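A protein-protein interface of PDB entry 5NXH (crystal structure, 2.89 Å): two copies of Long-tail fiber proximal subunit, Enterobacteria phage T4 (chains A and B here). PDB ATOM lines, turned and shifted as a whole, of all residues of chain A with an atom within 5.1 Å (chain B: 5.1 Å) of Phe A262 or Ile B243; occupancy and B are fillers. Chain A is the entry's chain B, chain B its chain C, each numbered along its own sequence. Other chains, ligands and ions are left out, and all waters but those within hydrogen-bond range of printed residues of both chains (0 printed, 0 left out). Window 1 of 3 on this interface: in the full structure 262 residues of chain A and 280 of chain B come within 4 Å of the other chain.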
ATOM      1  N   ILE A 243       5.719 -15.544 -19.549  1.00  0.00           N
ATOM      2  CA  ILE A 243       5.493 -16.747 -20.339  1.00  0.00           C
ATOM      3  C   ILE A 243       6.836 -17.470 -20.325  1.00  0.00           C
ATOM      4  O   ILE A 243       7.866 -16.834 -20.477  1.00  0.00           O
ATOM      5  CB  ILE A 243       5.071 -16.430 -21.793  1.00  0.00           C
ATOM      6  CG1 ILE A 243       3.886 -15.447 -21.823  1.00  0.00           C
ATOM      7  CG2 ILE A 243       4.667 -17.713 -22.506  1.00  0.00           C
ATOM      8  CD1 ILE A 243       3.462 -14.981 -23.203  1.00  0.00           C
ATOM      9  N   ARG A 244       6.826 -18.782 -20.119  1.00  0.00           N
ATOM     10  CA  ARG A 244       8.054 -19.576 -20.083  1.00  0.00           C
ATOM     11  C   ARG A 244       7.735 -20.979 -20.592  1.00  0.00           C
ATOM     12  O   ARG A 244       6.794 -21.603 -20.122  1.00  0.00           O
ATOM     13  CB  ARG A 244       8.649 -19.554 -18.660  1.00  0.00           C
ATOM     14  CG  ARG A 244       9.681 -20.624 -18.272  1.00  0.00           C
ATOM     15  CD  ARG A 244       9.843 -20.742 -16.748  1.00  0.00           C
ATOM     16  NE  ARG A 244      10.485 -22.016 -16.370  1.00  0.00           N
ATOM     17  CZ  ARG A 244      10.422 -22.615 -15.173  1.00  0.00           C
ATOM     18  NH1 ARG A 244       9.705 -22.101 -14.173  1.00  0.00           N
ATOM     19  NH2 ARG A 244      11.045 -23.780 -15.002  1.00  0.00           N
ATOM     20  N   VAL A 245       8.514 -21.454 -21.562  1.00  0.00           N
ATOM     21  CA  VAL A 245       8.313 -22.769 -22.172  1.00  0.00           C
ATOM     22  C   VAL A 245       9.412 -23.715 -21.722  1.00  0.00           C
ATOM     23  O   VAL A 245      10.580 -23.465 -22.009  1.00  0.00           O
ATOM     24  CB  VAL A 245       8.319 -22.669 -23.703  1.00  0.00           C
ATOM     25  CG1 VAL A 245       8.497 -24.042 -24.361  1.00  0.00           C
ATOM     26  CG2 VAL A 245       7.040 -21.986 -24.171  1.00  0.00           C
ATOM     27  N   THR A 260       6.586 -31.004 -22.393  1.00  0.00           N
ATOM     28  CA  THR A 260       6.535 -29.697 -23.048  1.00  0.00           C
ATOM     29  C   THR A 260       5.512 -28.818 -22.325  1.00  0.00           C
ATOM     30  O   THR A 260       4.333 -29.086 -22.408  1.00  0.00           O
ATOM     31  CB  THR A 260       6.122 -29.860 -24.531  1.00  0.00           C
ATOM     32  OG1 THR A 260       6.760 -31.020 -25.094  1.00  0.00           O
ATOM     33  CG2 THR A 260       6.481 -28.622 -25.338  1.00  0.00           C
ATOM     34  N   VAL A 261       5.954 -27.775 -21.625  1.00  0.00           N
ATOM     35  CA  VAL A 261       5.076 -26.960 -20.774  1.00  0.00           C
ATOM     36  C   VAL A 261       5.090 -25.476 -21.162  1.00  0.00           C
ATOM     37  O   VAL A 261       6.164 -24.882 -21.233  1.00  0.00           O
ATOM     38  CB  VAL A 261       5.534 -27.063 -19.308  1.00  0.00           C
ATOM     39  CG1 VAL A 261       4.709 -26.142 -18.399  1.00  0.00           C
ATOM     40  CG2 VAL A 261       5.493 -28.510 -18.817  1.00  0.00           C
ATOM     41  N   PHE A 262       3.907 -24.882 -21.363  1.00  0.00           N
ATOM     42  CA  PHE A 262       3.726 -23.448 -21.644  1.00  0.00           C
ATOM     43  C   PHE A 262       3.189 -22.794 -20.369  1.00  0.00           C
ATOM     44  O   PHE A 262       1.995 -22.787 -20.151  1.00  0.00           O
ATOM     45  CB  PHE A 262       2.717 -23.284 -22.792  1.00  0.00           C
ATOM     46  CG  PHE A 262       2.568 -21.875 -23.305  1.00  0.00           C
ATOM     47  CD1 PHE A 262       1.649 -20.995 -22.732  1.00  0.00           C
ATOM     48  CD2 PHE A 262       3.303 -21.444 -24.389  1.00  0.00           C
ATOM     49  CE1 PHE A 262       1.485 -19.707 -23.220  1.00  0.00           C
ATOM     50  CE2 PHE A 262       3.137 -20.155 -24.895  1.00  0.00           C
ATOM     51  CZ  PHE A 262       2.232 -19.280 -24.299  1.00  0.00           C
ATOM     52  N   GLU A 263       4.058 -22.267 -19.512  1.00  0.00           N
ATOM     53  CA  GLU A 263       3.647 -21.786 -18.180  1.00  0.00           C
ATOM     54  C   GLU A 263       3.611 -20.267 -18.133  1.00  0.00           C
ATOM     55  O   GLU A 263       4.620 -19.616 -18.333  1.00  0.00           O
ATOM     56  CB  GLU A 263       4.593 -22.369 -17.109  1.00  0.00           C
ATOM     57  CG  GLU A 263       4.314 -22.010 -15.637  1.00  0.00           C
ATOM     58  CD  GLU A 263       5.014 -22.942 -14.615  1.00  0.00           C
ATOM     59  OE1 GLU A 263       5.588 -23.999 -15.022  1.00  0.00           O
ATOM     60  OE2 GLU A 263       4.997 -22.601 -13.403  1.00  0.00           O
ATOM     61  N   VAL A 264       2.427 -19.706 -17.920  1.00  0.00           N
ATOM     62  CA  VAL A 264       2.261 -18.277 -17.678  1.00  0.00           C
ATOM     63  C   VAL A 264       2.106 -18.098 -16.170  1.00  0.00           C
ATOM     64  O   VAL A 264       1.232 -18.703 -15.569  1.00  0.00           O
ATOM     65  CB  VAL A 264       1.024 -17.711 -18.413  1.00  0.00           C
ATOM     66  CG1 VAL A 264       0.816 -16.230 -18.065  1.00  0.00           C
ATOM     67  CG2 VAL A 264       1.153 -17.922 -19.920  1.00  0.00           C
ATOM     68  N   PHE A 272      -1.541 -20.181 -14.954  1.00  0.00           N
ATOM     69  CA  PHE A 272      -1.958 -21.349 -15.709  1.00  0.00           C
ATOM     70  C   PHE A 272      -0.849 -21.917 -16.551  1.00  0.00           C
ATOM     71  O   PHE A 272       0.158 -21.256 -16.782  1.00  0.00           O
ATOM     72  CB  PHE A 272      -3.119 -20.998 -16.627  1.00  0.00           C
ATOM     73  CG  PHE A 272      -2.810 -19.951 -17.650  1.00  0.00           C
ATOM     74  CD1 PHE A 272      -3.027 -18.613 -17.371  1.00  0.00           C
ATOM     75  CD2 PHE A 272      -2.364 -20.305 -18.912  1.00  0.00           C
ATOM     76  CE1 PHE A 272      -2.780 -17.640 -18.327  1.00  0.00           C
ATOM     77  CE2 PHE A 272      -2.098 -19.336 -19.875  1.00  0.00           C
ATOM     78  CZ  PHE A 272      -2.314 -18.004 -19.583  1.00  0.00           C
ATOM     79  N   TYR A 273      -1.063 -23.139 -17.026  1.00  0.00           N
ATOM     80  CA  TYR A 273      -0.203 -23.722 -18.041  1.00  0.00           C
ATOM     81  C   TYR A 273      -0.891 -24.789 -18.854  1.00  0.00           C
ATOM     82  O   TYR A 273      -1.745 -25.485 -18.336  1.00  0.00           O
ATOM     83  CB  TYR A 273       1.050 -24.301 -17.403  1.00  0.00           C
ATOM     84  CG  TYR A 273       0.862 -25.527 -16.551  1.00  0.00           C
ATOM     85  CD1 TYR A 273       0.833 -26.798 -17.127  1.00  0.00           C
ATOM     86  CD2 TYR A 273       0.781 -25.433 -15.154  1.00  0.00           C
ATOM     87  CE1 TYR A 273       0.683 -27.938 -16.351  1.00  0.00           C
ATOM     88  CE2 TYR A 273       0.638 -26.572 -14.368  1.00  0.00           C
ATOM     89  CZ  TYR A 273       0.589 -27.817 -14.976  1.00  0.00           C
ATOM     90  OH  TYR A 273       0.445 -28.965 -14.244  1.00  0.00           O
ATOM     91  N   SER A 274      -0.527 -24.898 -20.124  1.00  0.00           N
ATOM     92  CA  SER A 274      -0.842 -26.074 -20.921  1.00  0.00           C
ATOM     93  C   SER A 274       0.405 -26.911 -20.907  1.00  0.00           C
ATOM     94  O   SER A 274       1.485 -26.374 -20.809  1.00  0.00           O
ATOM     95  CB  SER A 274      -1.200 -25.714 -22.366  1.00  0.00           C
ATOM     96  OG  SER A 274      -0.039 -25.509 -23.169  1.00  0.00           O
ATOM     97  N   GLN A 275       0.261 -28.223 -20.979  1.00  0.00           N
ATOM     98  CA  GLN A 275       1.400 -29.119 -21.130  1.00  0.00           C
ATOM     99  C   GLN A 275       1.025 -30.331 -21.966  1.00  0.00           C
ATOM    100  O   GLN A 275      -0.140 -30.623 -22.169  1.00  0.00           O
ATOM    101  CB  GLN A 275       1.976 -29.541 -19.767  1.00  0.00           C
ATOM    102  CG  GLN A 275       1.452 -30.837 -19.151  1.00  0.00           C
ATOM    103  CD  GLN A 275       2.092 -31.179 -17.803  1.00  0.00           C
ATOM    104  OE1 GLN A 275       2.788 -30.372 -17.187  1.00  0.00           O
ATOM    105  NE2 GLN A 275       1.850 -32.395 -17.345  1.00  0.00           N
ATOM    106  N   THR B 223       1.302 -13.488 -38.066  1.00  0.00           N
ATOM    107  CA  THR B 223       2.303 -13.192 -37.031  1.00  0.00           C
ATOM    108  C   THR B 223       2.516 -14.377 -36.091  1.00  0.00           C
ATOM    109  O   THR B 223       1.671 -15.253 -35.999  1.00  0.00           O
ATOM    110  CB  THR B 223       1.927 -11.963 -36.199  1.00  0.00           C
ATOM    111  OG1 THR B 223       0.645 -12.159 -35.601  1.00  0.00           O
ATOM    112  CG2 THR B 223       1.865 -10.747 -37.083  1.00  0.00           C
ATOM    113  N   SER B 224       3.650 -14.397 -35.401  1.00  0.00           N
ATOM    114  CA  SER B 224       4.056 -15.579 -34.649  1.00  0.00           C
ATOM    115  C   SER B 224       5.203 -15.302 -33.696  1.00  0.00           C
ATOM    116  O   SER B 224       6.081 -14.504 -33.998  1.00  0.00           O
ATOM    117  CB  SER B 224       4.477 -16.705 -35.600  1.00  0.00           C
ATOM    118  OG  SER B 224       5.286 -17.656 -34.937  1.00  0.00           O
ATOM    119  N   ILE B 225       5.189 -15.975 -32.548  1.00  0.00           N
ATOM    120  CA  ILE B 225       6.333 -16.022 -31.642  1.00  0.00           C
ATOM    121  C   ILE B 225       6.712 -17.488 -31.489  1.00  0.00           C
ATOM    122  O   ILE B 225       5.843 -18.336 -31.299  1.00  0.00           O
ATOM    123  CB  ILE B 225       6.004 -15.399 -30.258  1.00  0.00           C
ATOM    124  CG1 ILE B 225       5.762 -13.890 -30.389  1.00  0.00           C
ATOM    125  CG2 ILE B 225       7.124 -15.647 -29.243  1.00  0.00           C
ATOM    126  CD1 ILE B 225       5.511 -13.172 -29.073  1.00  0.00           C
ATOM    127  N   PHE B 227       9.240 -20.408 -29.471  1.00  0.00           N
ATOM    128  CA  PHE B 227       9.999 -20.744 -28.266  1.00  0.00           C
ATOM    129  C   PHE B 227      10.714 -22.058 -28.548  1.00  0.00           C
ATOM    130  O   PHE B 227      10.066 -23.091 -28.623  1.00  0.00           O
ATOM    131  CB  PHE B 227       9.046 -20.932 -27.076  1.00  0.00           C
ATOM    132  CG  PHE B 227       8.278 -19.703 -26.697  1.00  0.00           C
ATOM    133  CD1 PHE B 227       7.190 -19.286 -27.456  1.00  0.00           C
ATOM    134  CD2 PHE B 227       8.619 -18.973 -25.569  1.00  0.00           C
ATOM    135  CE1 PHE B 227       6.463 -18.172 -27.099  1.00  0.00           C
ATOM    136  CE2 PHE B 227       7.905 -17.851 -25.208  1.00  0.00           C
ATOM    137  CZ  PHE B 227       6.828 -17.451 -25.974  1.00  0.00           C
ATOM    138  N   MET B 241       7.503 -24.678 -29.055  1.00  0.00           N
ATOM    139  CA  MET B 241       6.165 -24.093 -28.946  1.00  0.00           C
ATOM    140  C   MET B 241       6.033 -22.840 -29.801  1.00  0.00           C
ATOM    141  O   MET B 241       7.032 -22.246 -30.218  1.00  0.00           O
ATOM    142  CB  MET B 241       5.897 -23.681 -27.500  1.00  0.00           C
ATOM    143  CG  MET B 241       5.744 -24.827 -26.513  1.00  0.00           C
ATOM    144  SD  MET B 241       4.005 -25.130 -26.214  1.00  0.00           S
ATOM    145  CE  MET B 241       4.166 -26.050 -24.685  1.00  0.00           C
ATOM    146  N   SER B 242       4.798 -22.412 -30.027  1.00  0.00           N
ATOM    147  CA  SER B 242       4.567 -21.166 -30.733  1.00  0.00           C
ATOM    148  C   SER B 242       3.215 -20.553 -30.446  1.00  0.00           C
ATOM    149  O   SER B 242       2.205 -21.235 -30.485  1.00  0.00           O
ATOM    150  CB  SER B 242       4.707 -21.379 -32.252  1.00  0.00           C
ATOM    151  OG  SER B 242       3.819 -22.380 -32.716  1.00  0.00           O
ATOM    152  N   ILE B 243       3.221 -19.255 -30.171  1.00  0.00           N
ATOM    153  CA  ILE B 243       2.012 -18.437 -30.212  1.00  0.00           C
ATOM    154  C   ILE B 243       1.891 -17.995 -31.660  1.00  0.00           C
ATOM    155  O   ILE B 243       2.887 -17.623 -32.258  1.00  0.00           O
ATOM    156  CB  ILE B 243       2.098 -17.205 -29.284  1.00  0.00           C
ATOM    157  CG1 ILE B 243       2.559 -17.589 -27.864  1.00  0.00           C
ATOM    158  CG2 ILE B 243       0.746 -16.526 -29.205  1.00  0.00           C
ATOM    159  CD1 ILE B 243       2.874 -16.388 -26.992  1.00  0.00           C
ATOM    160  N   ARG B 244       0.692 -18.063 -32.235  1.00  0.00           N
ATOM    161  CA  ARG B 244       0.474 -17.674 -33.634  1.00  0.00           C
ATOM    162  C   ARG B 244      -0.953 -17.156 -33.777  1.00  0.00           C
ATOM    163  O   ARG B 244      -1.886 -17.823 -33.365  1.00  0.00           O
ATOM    164  CB  ARG B 244       0.793 -18.862 -34.565  1.00  0.00           C
ATOM    165  CG  ARG B 244       0.276 -18.836 -36.012  1.00  0.00           C
ATOM    166  CD  ARG B 244       0.325 -20.227 -36.655  1.00  0.00           C
ATOM    167  NE  ARG B 244      -0.565 -20.348 -37.819  1.00  0.00           N
ATOM    168  CZ  ARG B 244      -1.072 -21.488 -38.316  1.00  0.00           C
ATOM    169  NH1 ARG B 244      -0.808 -22.675 -37.759  1.00  0.00           N
ATOM    170  NH2 ARG B 244      -1.887 -21.428 -39.373  1.00  0.00           N
ATOM    171  N   VAL B 245      -1.105 -15.969 -34.358  1.00  0.00           N
ATOM    172  CA  VAL B 245      -2.411 -15.341 -34.563  1.00  0.00           C
ATOM    173  C   VAL B 245      -2.783 -15.384 -36.036  1.00  0.00           C
ATOM    174  O   VAL B 245      -2.095 -14.789 -36.848  1.00  0.00           O
ATOM    175  CB  VAL B 245      -2.401 -13.883 -34.075  1.00  0.00           C
ATOM    176  CG1 VAL B 245      -3.600 -13.096 -34.595  1.00  0.00           C
ATOM    177  CG2 VAL B 245      -2.358 -13.856 -32.561  1.00  0.00           C
ATOM    178  N   PHE B 262      -6.112 -17.150 -31.864  1.00  0.00           N
ATOM    179  CA  PHE B 262      -4.897 -17.059 -31.039  1.00  0.00           C
ATOM    180  C   PHE B 262      -4.483 -18.495 -30.676  1.00  0.00           C
ATOM    181  O   PHE B 262      -4.960 -19.028 -29.714  1.00  0.00           O
ATOM    182  CB  PHE B 262      -5.203 -16.255 -29.770  1.00  0.00           C
ATOM    183  CG  PHE B 262      -3.998 -15.923 -28.922  1.00  0.00           C
ATOM    184  CD1 PHE B 262      -3.361 -14.707 -29.085  1.00  0.00           C
ATOM    185  CD2 PHE B 262      -3.523 -16.786 -27.922  1.00  0.00           C
ATOM    186  CE1 PHE B 262      -2.255 -14.358 -28.304  1.00  0.00           C
ATOM    187  CE2 PHE B 262      -2.417 -16.447 -27.158  1.00  0.00           C
ATOM    188  CZ  PHE B 262      -1.786 -15.234 -27.342  1.00  0.00           C
ATOM    189  N   GLU B 263      -3.612 -19.120 -31.454  1.00  0.00           N
ATOM    190  CA  GLU B 263      -3.303 -20.546 -31.293  1.00  0.00           C
ATOM    191  C   GLU B 263      -1.930 -20.722 -30.638  1.00  0.00           C
ATOM    192  O   GLU B 263      -0.923 -20.306 -31.193  1.00  0.00           O
ATOM    193  CB  GLU B 263      -3.392 -21.267 -32.661  1.00  0.00           C
ATOM    194  CG  GLU B 263      -3.079 -22.777 -32.700  1.00  0.00           C
ATOM    195  CD  GLU B 263      -3.460 -23.474 -34.025  1.00  0.00           C
ATOM    196  OE1 GLU B 263      -4.068 -22.878 -34.931  1.00  0.00           O
ATOM    197  OE2 GLU B 263      -3.184 -24.677 -34.178  1.00  0.00           O
ATOM    198  N   VAL B 264      -1.906 -21.312 -29.447  1.00  0.00           N
ATOM    199  CA  VAL B 264      -0.673 -21.750 -28.819  1.00  0.00           C
ATOM    200  C   VAL B 264      -0.532 -23.250 -29.074  1.00  0.00           C
ATOM    201  O   VAL B 264      -1.433 -24.009 -28.747  1.00  0.00           O
ATOM    202  CB  VAL B 264      -0.663 -21.454 -27.308  1.00  0.00           C
ATOM    203  CG1 VAL B 264       0.595 -22.025 -26.632  1.00  0.00           C
ATOM    204  CG2 VAL B 264      -0.767 -19.954 -27.053  1.00  0.00           C
ATOM    205  N   PHE B 272      -3.904 -25.231 -27.121  1.00  0.00           N
ATOM    206  CA  PHE B 272      -5.159 -24.515 -27.002  1.00  0.00           C
ATOM    207  C   PHE B 272      -5.234 -23.343 -27.942  1.00  0.00           C
ATOM    208  O   PHE B 272      -4.222 -22.904 -28.475  1.00  0.00           O
ATOM    209  CB  PHE B 272      -5.343 -24.000 -25.580  1.00  0.00           C
ATOM    210  CG  PHE B 272      -4.286 -23.030 -25.128  1.00  0.00           C
ATOM    211  CD1 PHE B 272      -4.466 -21.665 -25.305  1.00  0.00           C
ATOM    212  CD2 PHE B 272      -3.120 -23.478 -24.504  1.00  0.00           C
ATOM    213  CE1 PHE B 272      -3.521 -20.766 -24.866  1.00  0.00           C
ATOM    214  CE2 PHE B 272      -2.176 -22.585 -24.047  1.00  0.00           C
ATOM    215  CZ  PHE B 272      -2.381 -21.218 -24.228  1.00  0.00           C
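O of Ser A274 lies within hydrogen-bond range of N of Phe A262. N of Ile B225 lies within hydrogen-bond range of O of Ile B243 (2.8 Å). The backbone carbonyl oxygen (O) of Met B241 lies within hydrogen-bond range of the backbone NH (N) of Phe B227 (3.0 Å). The backbone NH (N) of Val B264 sits at hydrogen-bond distance from the backbone carbonyl oxygen (O) of Phe B272.
Among the printed residues, merely in contact across the chains: Thr A260 with Met B241, Phe A262 with Met B241, Phe A262 with Val B264, Val A245 with Met B241, Val A245 with Phe B227, Ser A274 with Phe B272, Val A261 with Met B241 and Phe A262 with Ile B243.
Printed residues of chain B within 4 Å of Thr A260: Met B241 (3.5 Å). Phe A262 touches three residues of chain B. Printed residues of chain B within 4 Å of Ser A274: Phe B272 (3.6 Å). Ile B243 touches just one residue of chain A: Phe A262. Printed residues of chain A within 4 Å of Phe B272: Ser A274 (3.6 Å).
Printed residues of chain B that touch a printed residue of chain A: Phe B227, Met B241, Ile B243, Val B264 and Phe B272. Hydrophobic or aromatic side chains of chain B within 4 Å of the printed part of chain A: Phe B227, Met B241, Ile B243, Val B264 and Phe B272. Along chain B the printed residues that touch a printed residue of chain A span positions 227 to 272. Of the 12 printed residues of chain A, 5 touch a printed residue of chain B. Hydrophobic or aromatic side chains of chain A within 4 Å of the printed part of chain B: Val A245 and Phe A262.
Phe A262 touches Ile B243, but with the chains exchanged Ile A243 does not touch Phe B262 (6.7 Å). Phe A262 touches Val B264, but with the chains exchanged Val A264 does not touch Phe B262 (8.2 Å). Positions printed for both chains: 243, 244, 245, 262, 263, 264 and 272. Of the 8 pairs that touch across the chains among the printed residues, none has its exchanged pair printed and touching as well.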
